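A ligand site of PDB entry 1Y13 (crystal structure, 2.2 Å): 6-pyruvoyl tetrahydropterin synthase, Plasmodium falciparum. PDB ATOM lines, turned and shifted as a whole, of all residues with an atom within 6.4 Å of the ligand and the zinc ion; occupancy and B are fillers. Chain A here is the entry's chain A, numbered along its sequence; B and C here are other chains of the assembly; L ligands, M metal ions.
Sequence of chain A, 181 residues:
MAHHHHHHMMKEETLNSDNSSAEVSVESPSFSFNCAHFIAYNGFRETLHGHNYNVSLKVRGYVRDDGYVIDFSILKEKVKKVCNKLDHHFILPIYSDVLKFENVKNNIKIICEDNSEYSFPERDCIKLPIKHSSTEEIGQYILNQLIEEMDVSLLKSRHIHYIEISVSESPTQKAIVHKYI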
ATOM      1  N   HIS A  37      15.788  15.354  11.466  1.00  0.00           N
ATOM      2  CA  HIS A  37      14.526  14.886  12.039  1.00  0.00           C
ATOM      3  C   HIS A  37      14.117  15.808  13.196  1.00  0.00           C
ATOM      4  O   HIS A  37      14.897  16.655  13.626  1.00  0.00           O
ATOM      5  CB  HIS A  37      14.667  13.419  12.540  1.00  0.00           C
ATOM      6  CG  HIS A  37      15.155  13.306  13.958  1.00  0.00           C
ATOM      7  ND1 HIS A  37      14.428  12.678  14.949  1.00  0.00           N
ATOM      8  CD2 HIS A  37      16.305  13.731  14.544  1.00  0.00           C
ATOM      9  CE1 HIS A  37      15.116  12.708  16.081  1.00  0.00           C
ATOM     10  NE2 HIS A  37      16.248  13.339  15.861  1.00  0.00           N
ATOM     11  N   PHE A  38      12.898  15.626  13.690  1.00  0.00           N
ATOM     12  CA  PHE A  38      12.571  16.132  15.001  1.00  0.00           C
ATOM     13  C   PHE A  38      11.557  15.188  15.608  1.00  0.00           C
ATOM     14  O   PHE A  38      10.733  14.612  14.910  1.00  0.00           O
ATOM     15  CB  PHE A  38      12.083  17.606  14.966  1.00  0.00           C
ATOM     16  CG  PHE A  38      10.831  17.830  14.158  1.00  0.00           C
ATOM     17  CD1 PHE A  38       9.594  17.669  14.735  1.00  0.00           C
ATOM     18  CD2 PHE A  38      10.901  18.219  12.824  1.00  0.00           C
ATOM     19  CE1 PHE A  38       8.414  17.881  13.984  1.00  0.00           C
ATOM     20  CE2 PHE A  38       9.761  18.442  12.082  1.00  0.00           C
ATOM     21  CZ  PHE A  38       8.511  18.258  12.643  1.00  0.00           C
ATOM     22  N   ILE A  39      11.675  14.985  16.913  1.00  0.00           N
ATOM     23  CA  ILE A  39      10.669  14.213  17.632  1.00  0.00           C
ATOM     24  C   ILE A  39       9.416  15.017  17.974  1.00  0.00           C
ATOM     25  O   ILE A  39       9.485  16.186  18.344  1.00  0.00           O
ATOM     26  CB  ILE A  39      11.302  13.503  18.836  1.00  0.00           C
ATOM     27  CG1 ILE A  39      11.938  12.198  18.328  1.00  0.00           C
ATOM     28  CG2 ILE A  39      10.259  13.225  19.912  1.00  0.00           C
ATOM     29  CD1 ILE A  39      13.117  11.744  19.118  1.00  0.00           C
ATOM     30  N   GLU A  46      10.121  19.130  19.370  1.00  0.00           N
ATOM     31  CA  GLU A  46      11.439  19.770  19.468  1.00  0.00           C
ATOM     32  C   GLU A  46      11.795  20.389  18.115  1.00  0.00           C
ATOM     33  O   GLU A  46      11.171  20.091  17.095  1.00  0.00           O
ATOM     34  CB  GLU A  46      12.532  18.767  19.914  1.00  0.00           C
ATOM     35  CG  GLU A  46      12.869  17.727  18.855  1.00  0.00           C
ATOM     36  CD  GLU A  46      13.717  16.555  19.358  1.00  0.00           C
ATOM     37  OE1 GLU A  46      14.170  16.561  20.523  1.00  0.00           O
ATOM     38  OE2 GLU A  46      13.934  15.618  18.554  1.00  0.00           O
ATOM     39  N   HIS A  49      16.744  19.204  13.873  1.00  0.00           N
ATOM     40  CA  HIS A  49      18.182  19.005  14.023  1.00  0.00           C
ATOM     41  C   HIS A  49      18.555  17.734  13.250  1.00  0.00           C
ATOM     42  O   HIS A  49      17.810  17.320  12.371  1.00  0.00           O
ATOM     43  CB  HIS A  49      18.600  18.932  15.500  1.00  0.00           C
ATOM     44  CG  HIS A  49      17.950  17.800  16.228  1.00  0.00           C
ATOM     45  ND1 HIS A  49      16.593  17.767  16.492  1.00  0.00           N
ATOM     46  CD2 HIS A  49      18.463  16.639  16.704  1.00  0.00           C
ATOM     47  CE1 HIS A  49      16.300  16.637  17.113  1.00  0.00           C
ATOM     48  NE2 HIS A  49      17.412  15.931  17.248  1.00  0.00           N
ATOM     49  N   GLY A  50      19.703  17.140  13.543  1.00  0.00           N
ATOM     50  CA  GLY A  50      20.138  15.967  12.803  1.00  0.00           C
ATOM     51  C   GLY A  50      21.138  15.125  13.540  1.00  0.00           C
ATOM     52  O   GLY A  50      21.611  15.504  14.588  1.00  0.00           O
ATOM     53  N   HIS A  51      21.448  13.967  12.959  1.00  0.00           N
ATOM     54  CA  HIS A  51      22.357  12.991  13.541  1.00  0.00           C
ATOM     55  C   HIS A  51      23.099  12.208  12.470  1.00  0.00           C
ATOM     56  O   HIS A  51      22.599  12.020  11.369  1.00  0.00           O
ATOM     57  CB  HIS A  51      21.592  11.985  14.415  1.00  0.00           C
ATOM     58  CG  HIS A  51      20.883  12.622  15.560  1.00  0.00           C
ATOM     59  ND1 HIS A  51      21.558  13.187  16.612  1.00  0.00           N
ATOM     60  CD2 HIS A  51      19.564  12.807  15.808  1.00  0.00           C
ATOM     61  CE1 HIS A  51      20.688  13.698  17.472  1.00  0.00           C
ATOM     62  NE2 HIS A  51      19.469  13.478  16.992  1.00  0.00           N
ATOM     63  N   TYR A  53      23.521   8.651  12.232  1.00  0.00           N
ATOM     64  CA  TYR A  53      23.057   7.415  12.843  1.00  0.00           C
ATOM     65  C   TYR A  53      23.964   6.301  12.394  1.00  0.00           C
ATOM     66  O   TYR A  53      24.420   6.292  11.244  1.00  0.00           O
ATOM     67  CB  TYR A  53      21.652   7.069  12.442  1.00  0.00           C
ATOM     68  CG  TYR A  53      20.575   8.012  12.891  1.00  0.00           C
ATOM     69  CD1 TYR A  53      20.207   9.119  12.093  1.00  0.00           C
ATOM     70  CD2 TYR A  53      19.855   7.762  14.065  1.00  0.00           C
ATOM     71  CE1 TYR A  53      19.165   9.960  12.489  1.00  0.00           C
ATOM     72  CE2 TYR A  53      18.816   8.596  14.454  1.00  0.00           C
ATOM     73  CZ  TYR A  53      18.459   9.694  13.655  1.00  0.00           C
ATOM     74  OH  TYR A  53      17.441  10.518  14.062  1.00  0.00           O
ATOM     75  N   SER A 133      10.123   9.528  14.819  1.00  0.00           N
ATOM     76  CA  SER A 133      11.486   9.343  14.350  1.00  0.00           C
ATOM     77  C   SER A 133      12.470   9.154  15.516  1.00  0.00           C
ATOM     78  O   SER A 133      13.540   9.760  15.554  1.00  0.00           O
ATOM     79  CB  SER A 133      11.932  10.500  13.429  1.00  0.00           C
ATOM     80  OG  SER A 133      11.818  11.747  14.098  1.00  0.00           O
ATOM     81  N   SER A 134      12.109   8.323  16.481  1.00  0.00           N
ATOM     82  CA  SER A 134      13.001   7.990  17.569  1.00  0.00           C
ATOM     83  C   SER A 134      13.931   6.909  17.078  1.00  0.00           C
ATOM     84  O   SER A 134      13.635   6.176  16.124  1.00  0.00           O
ATOM     85  CB  SER A 134      12.205   7.495  18.788  1.00  0.00           C
ATOM     86  OG  SER A 134      11.609   6.225  18.535  1.00  0.00           O
ATOM     87  N   THR A 135      15.064   6.797  17.745  1.00  0.00           N
ATOM     88  CA  THR A 135      16.098   5.808  17.471  1.00  0.00           C
ATOM     89  C   THR A 135      15.560   4.382  17.605  1.00  0.00           C
ATOM     90  O   THR A 135      15.846   3.531  16.753  1.00  0.00           O
ATOM     91  CB  THR A 135      17.315   6.090  18.424  1.00  0.00           C
ATOM     92  OG1 THR A 135      17.607   7.501  18.390  1.00  0.00           O
ATOM     93  CG2 THR A 135      18.536   5.388  17.964  1.00  0.00           C
ATOM     94  N   GLU A 136      14.772   4.128  18.658  1.00  0.00           N
ATOM     95  CA  GLU A 136      14.024   2.876  18.831  1.00  0.00           C
ATOM     96  C   GLU A 136      13.169   2.520  17.618  1.00  0.00           C
ATOM     97  O   GLU A 136      13.267   1.424  17.094  1.00  0.00           O
ATOM     98  CB  GLU A 136      13.115   2.917  20.073  1.00  0.00           C
ATOM     99  CG  GLU A 136      13.838   2.962  21.423  1.00  0.00           C
ATOM    100  CD  GLU A 136      13.997   4.383  21.936  1.00  0.00           C
ATOM    101  OE1 GLU A 136      14.289   5.286  21.113  1.00  0.00           O
ATOM    102  OE2 GLU A 136      13.808   4.607  23.164  1.00  0.00           O
ATOM    103  N   GLU A 169      22.173   7.108  17.798  1.00  0.00           N
ATOM    104  CA  GLU A 169      21.905   8.456  17.276  1.00  0.00           C
ATOM    105  C   GLU A 169      23.112   9.359  17.430  1.00  0.00           C
ATOM    106  O   GLU A 169      23.236  10.360  16.750  1.00  0.00           O
ATOM    107  CB  GLU A 169      20.637   9.073  17.874  1.00  0.00           C
ATOM    108  CG  GLU A 169      20.754   9.639  19.274  1.00  0.00           C
ATOM    109  CD  GLU A 169      19.610  10.621  19.610  1.00  0.00           C
ATOM    110  OE1 GLU A 169      18.508  10.542  19.008  1.00  0.00           O
ATOM    111  OE2 GLU A 169      19.838  11.502  20.485  1.00  0.00           O
ATOM    112  N   GLN A 173      24.597   7.545  22.793  1.00  0.00           N
ATOM    113  CA  GLN A 173      23.250   7.002  23.022  1.00  0.00           C
ATOM    114  C   GLN A 173      22.759   6.073  21.915  1.00  0.00           C
ATOM    115  O   GLN A 173      22.787   6.422  20.740  1.00  0.00           O
ATOM    116  CB  GLN A 173      22.236   8.117  23.315  1.00  0.00           C
ATOM    117  CG  GLN A 173      22.422   9.393  22.493  1.00  0.00           C
ATOM    118  CD  GLN A 173      21.787  10.621  23.154  1.00  0.00           C
ATOM    119  OE1 GLN A 173      22.017  10.899  24.330  1.00  0.00           O
ATOM    120  NE2 GLN A 173      20.995  11.361  22.390  1.00  0.00           N
ATOM    121  N   VAL B  24      17.662   0.658  25.588  1.00  0.00           N
ATOM    122  CA  VAL B  24      18.411   1.884  25.314  1.00  0.00           C
ATOM    123  C   VAL B  24      19.602   1.924  26.253  1.00  0.00           C
ATOM    124  O   VAL B  24      19.538   1.416  27.360  1.00  0.00           O
ATOM    125  CB  VAL B  24      17.557   3.184  25.446  1.00  0.00           C
ATOM    126  CG1 VAL B  24      16.605   3.325  24.263  1.00  0.00           C
ATOM    127  CG2 VAL B  24      16.775   3.208  26.743  1.00  0.00           C
ATOM    128  N   GLY B  67       7.300   7.087  21.804  1.00  0.00           N
ATOM    129  CA  GLY B  67       8.338   6.616  20.883  1.00  0.00           C
ATOM    130  C   GLY B  67       9.625   6.104  21.511  1.00  0.00           C
ATOM    131  O   GLY B  67      10.547   5.715  20.795  1.00  0.00           O
ATOM    132  N   TYR B  68       9.678   6.103  22.847  1.00  0.00           N
ATOM    133  CA  TYR B  68      10.906   5.807  23.591  1.00  0.00           C
ATOM    134  C   TYR B  68      10.749   4.578  24.457  1.00  0.00           C
ATOM    135  O   TYR B  68       9.659   4.290  24.916  1.00  0.00           O
ATOM    136  CB  TYR B  68      11.229   6.931  24.565  1.00  0.00           C
ATOM    137  CG  TYR B  68      11.497   8.273  23.984  1.00  0.00           C
ATOM    138  CD1 TYR B  68      12.036   8.412  22.692  1.00  0.00           C
ATOM    139  CD2 TYR B  68      11.258   9.421  24.725  1.00  0.00           C
ATOM    140  CE1 TYR B  68      12.304   9.662  22.155  1.00  0.00           C
ATOM    141  CE2 TYR B  68      11.525  10.701  24.191  1.00  0.00           C
ATOM    142  CZ  TYR B  68      12.042  10.804  22.903  1.00  0.00           C
ATOM    143  OH  TYR B  68      12.301  12.044  22.356  1.00  0.00           O
ATOM    144  N   VAL B  69      11.860   3.870  24.726  1.00  0.00           N
ATOM    145  CA  VAL B  69      11.886   2.972  25.891  1.00  0.00           C
ATOM    146  C   VAL B  69      11.812   3.882  27.142  1.00  0.00           C
ATOM    147  O   VAL B  69      10.959   3.691  28.010  1.00  0.00           O
ATOM    148  CB  VAL B  69      13.134   2.049  25.932  1.00  0.00           C
ATOM    149  CG1 VAL B  69      13.150   1.217  27.215  1.00  0.00           C
ATOM    150  CG2 VAL B  69      13.155   1.130  24.756  1.00  0.00           C
ATOM    151  N   ILE B  70      12.707   4.871  27.169  1.00  0.00           N
ATOM    152  CA  ILE B  70      12.729   5.991  28.117  1.00  0.00           C
ATOM    153  C   ILE B  70      13.623   7.063  27.478  1.00  0.00           C
ATOM    154  O   ILE B  70      14.539   6.729  26.719  1.00  0.00           O
ATOM    155  CB  ILE B  70      13.249   5.562  29.523  1.00  0.00           C
ATOM    156  CG1 ILE B  70      13.104   6.674  30.548  1.00  0.00           C
ATOM    157  CG2 ILE B  70      14.710   5.053  29.479  1.00  0.00           C
ATOM    158  CD1 ILE B  70      13.072   6.173  31.986  1.00  0.00           C
ATOM    159  N   ASP B  71      13.371   8.344  27.764  1.00  0.00           N
ATOM    160  CA  ASP B  71      14.160   9.436  27.196  1.00  0.00           C
ATOM    161  C   ASP B  71      15.654   9.288  27.561  1.00  0.00           C
ATOM    162  O   ASP B  71      15.990   9.077  28.717  1.00  0.00           O
ATOM    163  CB  ASP B  71      13.621  10.778  27.693  1.00  0.00           C
ATOM    164  CG  ASP B  71      14.041  11.963  26.820  1.00  0.00           C
ATOM    165  OD1 ASP B  71      15.201  12.040  26.352  1.00  0.00           O
ATOM    166  OD2 ASP B  71      13.175  12.853  26.603  1.00  0.00           O
ATOM    167  N   PHE B  72      16.540   9.398  26.555  1.00  0.00           N
ATOM    168  CA  PHE B  72      17.989   9.340  26.777  1.00  0.00           C
ATOM    169  C   PHE B  72      18.398  10.368  27.824  1.00  0.00           C
ATOM    170  O   PHE B  72      19.245  10.087  28.664  1.00  0.00           O
ATOM    171  CB  PHE B  72      18.804   9.608  25.499  1.00  0.00           C
ATOM    172  CG  PHE B  72      18.791   8.485  24.491  1.00  0.00           C
ATOM    173  CD1 PHE B  72      19.097   7.182  24.861  1.00  0.00           C
ATOM    174  CD2 PHE B  72      18.536   8.755  23.139  1.00  0.00           C
ATOM    175  CE1 PHE B  72      19.100   6.153  23.922  1.00  0.00           C
ATOM    176  CE2 PHE B  72      18.552   7.741  22.194  1.00  0.00           C
ATOM    177  CZ  PHE B  72      18.833   6.428  22.588  1.00  0.00           C
ATOM    178  N   SER B  73      17.801  11.559  27.767  1.00  0.00           N
ATOM    179  CA  SER B  73      18.165  12.677  28.672  1.00  0.00           C
ATOM    180  C   SER B  73      17.946  12.363  30.162  1.00  0.00           C
ATOM    181  O   SER B  73      18.708  12.845  31.010  1.00  0.00           O
ATOM    182  CB  SER B  73      17.416  13.951  28.295  1.00  0.00           C
ATOM    183  OG  SER B  73      16.026  13.803  28.512  1.00  0.00           O
ATOM    184  N   ASN C  34      24.220  18.880  17.559  1.00  0.00           N
ATOM    185  CA  ASN C  34      23.504  18.025  16.615  1.00  0.00           C
ATOM    186  C   ASN C  34      22.625  18.927  15.769  1.00  0.00           C
ATOM    187  O   ASN C  34      21.623  19.451  16.277  1.00  0.00           O
ATOM    188  CB  ASN C  34      22.670  16.953  17.348  1.00  0.00           C
ATOM    189  CG  ASN C  34      23.516  16.097  18.278  1.00  0.00           C
ATOM    190  OD1 ASN C  34      24.739  16.029  18.164  1.00  0.00           O
ATOM    191  ND2 ASN C  34      22.868  15.451  19.212  1.00  0.00           N
ATOM    192  N   HIS C  88      20.986  21.607  18.248  1.00  0.00           N
ATOM    193  CA  HIS C  88      19.567  21.445  17.941  1.00  0.00           C
ATOM    194  C   HIS C  88      18.944  22.513  17.057  1.00  0.00           C
ATOM    195  O   HIS C  88      17.841  22.961  17.324  1.00  0.00           O
ATOM    196  CB  HIS C  88      18.745  21.288  19.211  1.00  0.00           C
ATOM    197  CG  HIS C  88      18.616  19.870  19.646  1.00  0.00           C
ATOM    198  ND1 HIS C  88      17.409  19.197  19.664  1.00  0.00           N
ATOM    199  CD2 HIS C  88      19.550  18.964  20.040  1.00  0.00           C
ATOM    200  CE1 HIS C  88      17.605  17.958  20.069  1.00  0.00           C
ATOM    201  NE2 HIS C  88      18.895  17.792  20.301  1.00  0.00           N
HETATM  202  N1  LIG L   1      15.330   9.291  23.613  1.00  0.00           N
HETATM  203  N2  LIG L   1      14.978   7.002  23.808  1.00  0.00           N
HETATM  204  C1  LIG L   1      15.194   8.092  23.022  1.00  0.00           C
HETATM  205  N3  LIG L   1      15.274   8.032  21.673  1.00  0.00           N
HETATM  206  C2  LIG L   1      15.637  10.420  21.407  1.00  0.00           C
HETATM  207  C3  LIG L   1      15.541  10.431  22.879  1.00  0.00           C
HETATM  208  N4  LIG L   1      15.658  11.635  23.512  1.00  0.00           N
HETATM  209  C4  LIG L   1      15.864  12.791  22.844  1.00  0.00           C
HETATM  210  C5  LIG L   1      15.980  12.787  21.469  1.00  0.00           C
HETATM  211  N5  LIG L   1      15.850  11.607  20.799  1.00  0.00           N
HETATM  212  C6  LIG L   1      16.207  14.079  20.707  1.00  0.00           C
HETATM  213  O1  LIG L   1      15.657  14.030  19.331  1.00  0.00           O
HETATM  214  C7  LIG L   1      17.705  14.527  20.659  1.00  0.00           C
HETATM  215  O2  LIG L   1      18.359  14.051  19.460  1.00  0.00           O
HETATM  216  C8  LIG L   1      18.582  14.147  21.869  1.00  0.00           C
HETATM  217 ZN    ZN M   1      17.401  13.868  17.773  1.00  0.00          ZN
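OD1 of Asp 71 of chain B sits close to N4 of the ligand, at 2.9 Å. Residues that only touch the ligand: Tyr 68 of chain B, Ile 39, His 88 of chain C and Gln 173. Hydrophobic or aromatic side chains within 4 Å of the ligand: His 37, Ile 39, His 49, His 51, Tyr 68 of chain B, Phe 72 of chain B and His 88 of chain C. Within 4 Å of the ligand: His 37, Ile 39, Glu 46, His 49, His 51, Glu 136, Glu 169, Gln 173, Tyr 68 of chain B, Ile 70 of chain B, Asp 71 of chain B, Phe 72 of chain B and His 88 of chain C.
The zinc ion is bound by an oxygen (O2) of the ligand (1.9 Å), a ring nitrogen (NE2) of His 49 (2.1 Å), a ring nitrogen (NE2) of His 51 (2.2 Å), a ring nitrogen (NE2) of His 37 (2.3 Å) and an oxygen (O1) of the ligand (2.3 Å). The zinc ion has five donor atoms within binding distance.
O1 of the ligand sits close to OE2 of Glu 46, 2.5 Å away. The side-chain carboxylate of Glu 136 lies within hydrogen-bond range of a nitrogen (N2) of the ligand, 2.7 Å away. The backbone carbonyl oxygen of Ile 70 of chain B lies within hydrogen-bond range of a nitrogen (N2) of the ligand, at 3.0 Å. The side-chain carboxylate (OE2) of Glu 169 sits close to an oxygen (O2) of the ligand, 3.1 Å away. The backbone NH of Phe 72 of chain B sits at hydrogen-bond distance from a nitrogen (N1) of the ligand, 3.2 Å away.
OE2 of Glu 46 touches the zinc ion, 3.96 Å away. Glu 169 touches the zinc ion. Five residues have an atom within 4 Å of the zinc ion: His 37, Glu 46, His 49, His 51 and Glu 169. Along chain A the residues within 4 Å of the zinc ion span positions 37 to 169.
A ring nitrogen (ND1) of His 51 sits close to the backbone carbonyl oxygen (O) of Glu 169. ND1 of His 37 sits at hydrogen-bond distance from OG of Ser 133. The side-chain carboxylate of Glu 46 sits at hydrogen-bond distance from the backbone NH of Ile 39 (2.9 Å). OE2 of Glu 136 sits at hydrogen-bond distance from N of Val 69 of chain B (2.6 Å). OD1 of Asp 71 of chain B sits at hydrogen-bond distance from OG of Ser 73 of chain B (2.9 Å). The side-chain hydroxyl of Thr 135 lies within hydrogen-bond range of the side-chain carboxylate of Glu 169 (3.2 Å). The backbone NH (N) of His 88 of chain C sits at hydrogen-bond distance from the backbone carbonyl oxygen (O) of Asn 34 of chain C (3.0 Å).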
